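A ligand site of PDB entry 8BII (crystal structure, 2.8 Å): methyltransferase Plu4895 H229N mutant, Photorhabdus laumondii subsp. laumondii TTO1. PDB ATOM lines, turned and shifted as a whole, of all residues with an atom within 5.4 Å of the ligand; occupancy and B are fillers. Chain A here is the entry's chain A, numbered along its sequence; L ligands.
O of Phe 144 is in hydrogen-bond range of NH1 of Arg 212.
The backbone carbonyl oxygen of Leu 210 sits at hydrogen-bond distance from the backbone NH of Gly 188 (2.7 Å).
ND2 of Asn 244 sits close to NZ of Lys 243 (3.5 Å).
The side-chain amino group (NZ) of Lys 243 is in hydrogen-bond range of the side-chain hydroxyl (OG1) of Thr 165 (2.6 Å).
N of Gly 190 sits at hydrogen-bond distance from OD2 of Asp 211, at 2.9 Å.
ND2 of Asn 248 sits close to O of Val 245, at 3.5 Å.
O of Met 161 is in hydrogen-bond range of OG1 of Thr 165, 3.1 Å away.
The backbone NH (N) of Phe 230 sits at hydrogen-bond distance from the side-chain carboxylate (OD2) of Asp 228 (3.0 Å).
Merely in contact with the ligand: Phe 144 (3.6 Å), Phe 157 (3.8 Å), Met 161 (3.6 Å), Gly 189 (3.7 Å), Gly 190 (3.6 Å), Arg 212 (3.5 Å), Phe 230 (3.7 Å), Asn 248 (3.3 Å) and Trp 249 (3.6 Å).
Hydrophobic or aromatic side chains within 4 Å of the ligand: Phe 144, Phe 157, Met 161, Phe 229, Phe 230 and Trp 249.
16 residues have an atom within 4 Å of the ligand: Phe 144, Phe 157, Met 161, Thr 165, Gly 188, Gly 189, Gly 190, Asp 211, Arg 212, Asp 228, Phe 229, Phe 230, Lys 243, Asn 244, Asn 248 and Trp 249.
The nearest printed residue that does not touch the ligand is Leu 210 (4.2 Å).
N of Phe 229 is in hydrogen-bond range of N5 of the ligand, at 3.4 Å.
The backbone carbonyl oxygen (O) of Lys 243 sits at hydrogen-bond distance from a nitrogen (N1) of the ligand, at 2.8 Å.
NZ of Lys 243 lies within salt-bridge range of O2 of the ligand.
The side-chain hydroxyl of Thr 165 sits at hydrogen-bond distance from an oxygen (O1) of the ligand (3.3 Å).
O of Gly 188 sits at hydrogen-bond distance from N1 of the ligand, 2.9 Å away.
O2 of the ligand is in hydrogen-bond range of ND2 of Asn 244 (3.2 Å).
A nitrogen (N4) of the ligand lies within hydrogen-bond range of the side-chain carboxylate (OD2) of Asp 228, 3.0 Å away.
O5 of the ligand sits at hydrogen-bond distance from OD1 of Asp 211.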
ATOM      1  N   PHE A 144      10.394   9.835  -8.312  1.00  0.00           N
ATOM      2  CA  PHE A 144      11.695  10.306  -7.762  1.00  0.00           C
ATOM      3  C   PHE A 144      12.183  11.547  -8.543  1.00  0.00           C
ATOM      4  O   PHE A 144      12.839  12.409  -7.924  1.00  0.00           O
ATOM      5  CB  PHE A 144      12.709   9.173  -7.754  1.00  0.00           C
ATOM      6  CG  PHE A 144      12.439   8.121  -6.709  1.00  0.00           C
ATOM      7  CD1 PHE A 144      12.376   8.460  -5.366  1.00  0.00           C
ATOM      8  CD2 PHE A 144      12.237   6.791  -7.062  1.00  0.00           C
ATOM      9  CE1 PHE A 144      12.115   7.499  -4.399  1.00  0.00           C
ATOM     10  CE2 PHE A 144      11.990   5.830  -6.096  1.00  0.00           C
ATOM     11  CZ  PHE A 144      11.925   6.189  -4.768  1.00  0.00           C
ATOM     12  N   LYS A 154       9.726  15.651  -0.450  1.00  0.00           N
ATOM     13  CA  LYS A 154      10.974  14.841  -0.308  1.00  0.00           C
ATOM     14  C   LYS A 154      11.317  14.726   1.185  1.00  0.00           C
ATOM     15  O   LYS A 154      11.589  13.596   1.649  1.00  0.00           O
ATOM     16  CB  LYS A 154      12.138  15.475  -1.081  1.00  0.00           C
ATOM     17  CG  LYS A 154      13.091  14.489  -1.748  1.00  0.00           C
ATOM     18  CD  LYS A 154      14.027  13.772  -0.793  1.00  0.00           C
ATOM     19  CE  LYS A 154      14.760  12.631  -1.450  1.00  0.00           C
ATOM     20  NZ  LYS A 154      15.653  11.926  -0.487  1.00  0.00           N
ATOM     21  N   PHE A 157       8.779  12.527   2.839  1.00  0.00           N
ATOM     22  CA  PHE A 157       9.064  11.132   2.409  1.00  0.00           C
ATOM     23  C   PHE A 157      10.217  10.562   3.257  1.00  0.00           C
ATOM     24  O   PHE A 157      10.056   9.467   3.824  1.00  0.00           O
ATOM     25  CB  PHE A 157       9.398  11.078   0.922  1.00  0.00           C
ATOM     26  CG  PHE A 157       9.815   9.723   0.416  1.00  0.00           C
ATOM     27  CD1 PHE A 157       8.870   8.728   0.189  1.00  0.00           C
ATOM     28  CD2 PHE A 157      11.147   9.430   0.159  1.00  0.00           C
ATOM     29  CE1 PHE A 157       9.251   7.487  -0.278  1.00  0.00           C
ATOM     30  CE2 PHE A 157      11.520   8.182  -0.309  1.00  0.00           C
ATOM     31  CZ  PHE A 157      10.576   7.214  -0.528  1.00  0.00           C
ATOM     32  N   MET A 161      10.056   7.526   6.060  1.00  0.00           N
ATOM     33  CA  MET A 161      10.960   6.367   5.809  1.00  0.00           C
ATOM     34  C   MET A 161      11.896   6.167   7.007  1.00  0.00           C
ATOM     35  O   MET A 161      12.235   5.006   7.284  1.00  0.00           O
ATOM     36  CB  MET A 161      11.773   6.579   4.537  1.00  0.00           C
ATOM     37  CG  MET A 161      10.934   6.528   3.272  1.00  0.00           C
ATOM     38  SD  MET A 161      10.402   4.838   2.869  1.00  0.00           S
ATOM     39  CE  MET A 161       8.663   5.105   2.544  1.00  0.00           C
ATOM     40  N   SER A 162      12.286   7.249   7.693  1.00  0.00           N
ATOM     41  CA  SER A 162      13.131   7.219   8.911  1.00  0.00           C
ATOM     42  C   SER A 162      12.428   6.435  10.026  1.00  0.00           C
ATOM     43  O   SER A 162      13.122   5.700  10.762  1.00  0.00           O
ATOM     44  CB  SER A 162      13.471   8.614   9.394  1.00  0.00           C
ATOM     45  OG  SER A 162      14.204   9.331   8.402  1.00  0.00           O
ATOM     46  N   THR A 165      12.483   2.703   9.338  1.00  0.00           N
ATOM     47  CA  THR A 165      13.894   2.267   9.576  1.00  0.00           C
ATOM     48  C   THR A 165      14.090   1.984  11.077  1.00  0.00           C
ATOM     49  O   THR A 165      14.732   0.957  11.391  1.00  0.00           O
ATOM     50  CB  THR A 165      14.889   3.323   9.078  1.00  0.00           C
ATOM     51  OG1 THR A 165      14.790   3.370   7.652  1.00  0.00           O
ATOM     52  CG2 THR A 165      16.318   3.034   9.485  1.00  0.00           C
ATOM     53  N   ASP A 186      24.943   0.986   1.343  1.00  0.00           N
ATOM     54  CA  ASP A 186      23.463   1.015   1.294  1.00  0.00           C
ATOM     55  C   ASP A 186      23.034   1.623  -0.048  1.00  0.00           C
ATOM     56  O   ASP A 186      23.111   2.857  -0.184  1.00  0.00           O
ATOM     57  CB  ASP A 186      22.874   1.784   2.493  1.00  0.00           C
ATOM     58  CG  ASP A 186      21.381   1.595   2.694  1.00  0.00           C
ATOM     59  OD1 ASP A 186      20.768   0.833   1.921  1.00  0.00           O
ATOM     60  OD2 ASP A 186      20.836   2.215   3.632  1.00  0.00           O
ATOM     61  N   LEU A 187      22.613   0.777  -0.996  1.00  0.00           N
ATOM     62  CA  LEU A 187      22.136   1.191  -2.339  1.00  0.00           C
ATOM     63  C   LEU A 187      20.720   1.772  -2.205  1.00  0.00           C
ATOM     64  O   LEU A 187      19.805   1.015  -1.836  1.00  0.00           O
ATOM     65  CB  LEU A 187      22.147  -0.024  -3.271  1.00  0.00           C
ATOM     66  CG  LEU A 187      23.512  -0.665  -3.501  1.00  0.00           C
ATOM     67  CD1 LEU A 187      23.357  -2.046  -4.117  1.00  0.00           C
ATOM     68  CD2 LEU A 187      24.386   0.215  -4.365  1.00  0.00           C
ATOM     69  N   GLY A 188      20.567   3.076  -2.482  1.00  0.00           N
ATOM     70  CA  GLY A 188      19.298   3.817  -2.306  1.00  0.00           C
ATOM     71  C   GLY A 188      18.943   3.966  -0.840  1.00  0.00           C
ATOM     72  O   GLY A 188      17.852   3.505  -0.454  1.00  0.00           O
ATOM     73  N   GLY A 189      19.819   4.599  -0.064  1.00  0.00           N
ATOM     74  CA  GLY A 189      19.684   4.759   1.400  1.00  0.00           C
ATOM     75  C   GLY A 189      19.296   6.174   1.806  1.00  0.00           C
ATOM     76  O   GLY A 189      19.364   6.469   3.015  1.00  0.00           O
ATOM     77  N   GLY A 190      18.894   7.022   0.840  1.00  0.00           N
ATOM     78  CA  GLY A 190      18.476   8.416   1.074  1.00  0.00           C
ATOM     79  C   GLY A 190      19.335   9.095   2.129  1.00  0.00           C
ATOM     80  O   GLY A 190      20.569   9.056   2.005  1.00  0.00           O
ATOM     81  N   LEU A 210      24.848   5.143  -1.149  1.00  0.00           N
ATOM     82  CA  LEU A 210      24.734   5.489  -2.587  1.00  0.00           C
ATOM     83  C   LEU A 210      23.283   5.864  -2.892  1.00  0.00           C
ATOM     84  O   LEU A 210      22.385   5.059  -2.581  1.00  0.00           O
ATOM     85  CB  LEU A 210      25.187   4.290  -3.429  1.00  0.00           C
ATOM     86  CG  LEU A 210      25.334   4.563  -4.931  1.00  0.00           C
ATOM     87  CD1 LEU A 210      26.417   3.676  -5.530  1.00  0.00           C
ATOM     88  CD2 LEU A 210      24.015   4.371  -5.667  1.00  0.00           C
ATOM     89  N   ASP A 211      23.067   7.049  -3.482  1.00  0.00           N
ATOM     90  CA  ASP A 211      21.722   7.540  -3.890  1.00  0.00           C
ATOM     91  C   ASP A 211      21.891   8.776  -4.793  1.00  0.00           C
ATOM     92  O   ASP A 211      22.885   9.508  -4.622  1.00  0.00           O
ATOM     93  CB  ASP A 211      20.850   7.860  -2.668  1.00  0.00           C
ATOM     94  CG  ASP A 211      19.363   7.754  -2.927  1.00  0.00           C
ATOM     95  OD1 ASP A 211      18.925   8.154  -4.027  1.00  0.00           O
ATOM     96  OD2 ASP A 211      18.646   7.265  -2.025  1.00  0.00           O
ATOM     97  N   ARG A 212      20.941   8.976  -5.705  1.00  0.00           N
ATOM     98  CA  ARG A 212      20.836  10.168  -6.600  1.00  0.00           C
ATOM     99  C   ARG A 212      20.459  11.404  -5.756  1.00  0.00           C
ATOM    100  O   ARG A 212      19.268  11.563  -5.441  1.00  0.00           O
ATOM    101  CB  ARG A 212      19.823   9.920  -7.716  1.00  0.00           C
ATOM    102  CG  ARG A 212      18.518   9.287  -7.263  1.00  0.00           C
ATOM    103  CD  ARG A 212      17.601   8.892  -8.403  1.00  0.00           C
ATOM    104  NE  ARG A 212      17.047  10.025  -9.127  1.00  0.00           N
ATOM    105  CZ  ARG A 212      16.131  10.858  -8.659  1.00  0.00           C
ATOM    106  NH1 ARG A 212      15.694  11.852  -9.408  1.00  0.00           N
ATOM    107  NH2 ARG A 212      15.652  10.721  -7.424  1.00  0.00           N
ATOM    108  N   GLY A 227      25.507   8.619  -6.864  1.00  0.00           N
ATOM    109  CA  GLY A 227      25.589   7.586  -7.928  1.00  0.00           C
ATOM    110  C   GLY A 227      24.234   7.144  -8.431  1.00  0.00           C
ATOM    111  O   GLY A 227      23.244   7.879  -8.248  1.00  0.00           O
ATOM    112  N   ASP A 228      24.196   5.962  -9.063  1.00  0.00           N
ATOM    113  CA  ASP A 228      23.003   5.364  -9.728  1.00  0.00           C
ATOM    114  C   ASP A 228      23.209   3.852  -9.805  1.00  0.00           C
ATOM    115  O   ASP A 228      24.219   3.432 -10.410  1.00  0.00           O
ATOM    116  CB  ASP A 228      22.782   6.001 -11.106  1.00  0.00           C
ATOM    117  CG  ASP A 228      21.617   5.430 -11.903  1.00  0.00           C
ATOM    118  OD1 ASP A 228      21.414   5.889 -13.043  1.00  0.00           O
ATOM    119  OD2 ASP A 228      20.916   4.546 -11.376  1.00  0.00           O
ATOM    120  N   PHE A 229      22.279   3.058  -9.245  1.00  0.00           N
ATOM    121  CA  PHE A 229      22.403   1.573  -9.126  1.00  0.00           C
ATOM    122  C   PHE A 229      21.988   0.889 -10.434  1.00  0.00           C
ATOM    123  O   PHE A 229      22.042  -0.355 -10.475  1.00  0.00           O
ATOM    124  CB  PHE A 229      21.649   1.044  -7.905  1.00  0.00           C
ATOM    125  CG  PHE A 229      20.217   1.503  -7.713  1.00  0.00           C
ATOM    126  CD1 PHE A 229      19.312   1.516  -8.761  1.00  0.00           C
ATOM    127  CD2 PHE A 229      19.774   1.877  -6.452  1.00  0.00           C
ATOM    128  CE1 PHE A 229      18.004   1.925  -8.566  1.00  0.00           C
ATOM    129  CE2 PHE A 229      18.459   2.278  -6.259  1.00  0.00           C
ATOM    130  CZ  PHE A 229      17.582   2.307  -7.305  1.00  0.00           C
ATOM    131  N   PHE A 230      21.576   1.657 -11.456  1.00  0.00           N
ATOM    132  CA  PHE A 230      21.350   1.171 -12.841  1.00  0.00           C
ATOM    133  C   PHE A 230      22.681   1.162 -13.610  1.00  0.00           C
ATOM    134  O   PHE A 230      22.780   0.456 -14.628  1.00  0.00           O
ATOM    135  CB  PHE A 230      20.290   2.008 -13.566  1.00  0.00           C
ATOM    136  CG  PHE A 230      18.874   1.677 -13.165  1.00  0.00           C
ATOM    137  CD1 PHE A 230      18.322   0.433 -13.429  1.00  0.00           C
ATOM    138  CD2 PHE A 230      18.076   2.630 -12.526  1.00  0.00           C
ATOM    139  CE1 PHE A 230      17.028   0.131 -13.065  1.00  0.00           C
ATOM    140  CE2 PHE A 230      16.776   2.321 -12.164  1.00  0.00           C
ATOM    141  CZ  PHE A 230      16.252   1.078 -12.431  1.00  0.00           C
ATOM    142  N   LYS A 243      17.394  -1.827   0.900  1.00  0.00           N
ATOM    143  CA  LYS A 243      16.260  -1.677   1.847  1.00  0.00           C
ATOM    144  C   LYS A 243      15.171  -0.813   1.198  1.00  0.00           C
ATOM    145  O   LYS A 243      15.421   0.391   1.001  1.00  0.00           O
ATOM    146  CB  LYS A 243      16.730  -1.078   3.166  1.00  0.00           C
ATOM    147  CG  LYS A 243      15.645  -0.852   4.204  1.00  0.00           C
ATOM    148  CD  LYS A 243      16.158  -0.370   5.544  1.00  0.00           C
ATOM    149  CE  LYS A 243      15.058   0.012   6.506  1.00  0.00           C
ATOM    150  NZ  LYS A 243      14.403   1.279   6.108  1.00  0.00           N
ATOM    151  N   ASN A 244      14.027  -1.411   0.875  1.00  0.00           N
ATOM    152  CA  ASN A 244      12.815  -0.743   0.327  1.00  0.00           C
ATOM    153  C   ASN A 244      13.181  -0.030  -0.981  1.00  0.00           C
ATOM    154  O   ASN A 244      12.854   1.164  -1.124  1.00  0.00           O
ATOM    155  CB  ASN A 244      12.207   0.218   1.356  1.00  0.00           C
ATOM    156  CG  ASN A 244      11.750  -0.481   2.616  1.00  0.00           C
ATOM    157  OD1 ASN A 244      11.023  -1.468   2.567  1.00  0.00           O
ATOM    158  ND2 ASN A 244      12.163   0.039   3.759  1.00  0.00           N
ATOM    159  N   VAL A 245      13.839  -0.750  -1.900  1.00  0.00           N
ATOM    160  CA  VAL A 245      14.276  -0.242  -3.237  1.00  0.00           C
ATOM    161  C   VAL A 245      13.576  -1.055  -4.331  1.00  0.00           C
ATOM    162  O   VAL A 245      12.853  -0.462  -5.138  1.00  0.00           O
ATOM    163  CB  VAL A 245      15.808  -0.314  -3.386  1.00  0.00           C
ATOM    164  CG1 VAL A 245      16.268  -0.011  -4.800  1.00  0.00           C
ATOM    165  CG2 VAL A 245      16.500   0.612  -2.394  1.00  0.00           C
ATOM    166  N   ASN A 248      10.160  -0.662  -5.748  1.00  0.00           N
ATOM    167  CA  ASN A 248       9.932   0.553  -6.580  1.00  0.00           C
ATOM    168  C   ASN A 248      10.229   0.264  -8.050  1.00  0.00           C
ATOM    169  O   ASN A 248      10.209   1.227  -8.847  1.00  0.00           O
ATOM    170  CB  ASN A 248      10.785   1.733  -6.117  1.00  0.00           C
ATOM    171  CG  ASN A 248      10.780   1.945  -4.620  1.00  0.00           C
ATOM    172  OD1 ASN A 248       9.899   1.456  -3.920  1.00  0.00           O
ATOM    173  ND2 ASN A 248      11.764   2.679  -4.121  1.00  0.00           N
ATOM    174  N   TRP A 249      10.485  -1.003  -8.416  1.00  0.00           N
ATOM    175  CA  TRP A 249      10.993  -1.397  -9.754  1.00  0.00           C
ATOM    176  C   TRP A 249      10.343  -2.691 -10.223  1.00  0.00           C
ATOM    177  O   TRP A 249      10.274  -3.657  -9.469  1.00  0.00           O
ATOM    178  CB  TRP A 249      12.525  -1.518  -9.718  1.00  0.00           C
ATOM    179  CG  TRP A 249      13.186  -0.245  -9.279  1.00  0.00           C
ATOM    180  CD1 TRP A 249      13.804  -0.020  -8.082  1.00  0.00           C
ATOM    181  CD2 TRP A 249      13.253   0.986 -10.003  1.00  0.00           C
ATOM    182  NE1 TRP A 249      14.269   1.265  -8.026  1.00  0.00           N
ATOM    183  CE2 TRP A 249      13.941   1.908  -9.191  1.00  0.00           C
ATOM    184  CE3 TRP A 249      12.806   1.399 -11.266  1.00  0.00           C
ATOM    185  CZ2 TRP A 249      14.187   3.214  -9.598  1.00  0.00           C
ATOM    186  CZ3 TRP A 249      13.045   2.695 -11.665  1.00  0.00           C
ATOM    187  CH2 TRP A 249      13.736   3.584 -10.842  1.00  0.00           C
HETATM  188  N1  LIG L   1      16.648   2.697   2.007  1.00  0.00           N
HETATM  189  C1  LIG L   1      15.896   3.898   2.516  1.00  0.00           C
HETATM  190  C2  LIG L   1      15.163   4.622   1.382  1.00  0.00           C
HETATM  191  C3  LIG L   1      14.393   3.688   0.460  1.00  0.00           C
HETATM  192  S1  LIG L   1      13.257   4.573  -0.641  1.00  0.00           S
HETATM  193  C4  LIG L   1      14.881   3.444   3.580  1.00  0.00           C
HETATM  194  O1  LIG L   1      14.540   4.210   4.486  1.00  0.00           O
HETATM  195  O2  LIG L   1      14.390   2.322   3.546  1.00  0.00           O
HETATM  196  C5  LIG L   1      14.013   4.315  -2.261  1.00  0.00           C
HETATM  197  C6  LIG L   1      15.310   5.061  -2.458  1.00  0.00           C
HETATM  198  O3  LIG L   1      15.861   4.732  -3.760  1.00  0.00           O
HETATM  199  C7  LIG L   1      15.186   6.586  -2.417  1.00  0.00           C
HETATM  200  O4  LIG L   1      16.051   7.133  -1.435  1.00  0.00           O
HETATM  201  C8  LIG L   1      15.590   7.027  -3.824  1.00  0.00           C
HETATM  202  O5  LIG L   1      16.292   8.251  -3.847  1.00  0.00           O
HETATM  203  C9  LIG L   1      16.497   5.884  -4.249  1.00  0.00           C
HETATM  204  N2  LIG L   1      16.682   5.754  -5.690  1.00  0.00           N
HETATM  205  C10 LIG L   1      15.711   5.831  -6.658  1.00  0.00           C
HETATM  206  N3  LIG L   1      16.184   5.687  -7.873  1.00  0.00           N
HETATM  207  C11 LIG L   1      17.541   5.499  -7.700  1.00  0.00           C
HETATM  208  C12 LIG L   1      18.596   5.291  -8.603  1.00  0.00           C
HETATM  209  N4  LIG L   1      18.435   5.224  -9.931  1.00  0.00           N
HETATM  210  N5  LIG L   1      19.851   5.140  -8.101  1.00  0.00           N
HETATM  211  C13 LIG L   1      19.998   5.206  -6.772  1.00  0.00           C
HETATM  212  N6  LIG L   1      19.091   5.400  -5.817  1.00  0.00           N
HETATM  213  C14 LIG L   1      17.869   5.541  -6.357  1.00  0.00           C
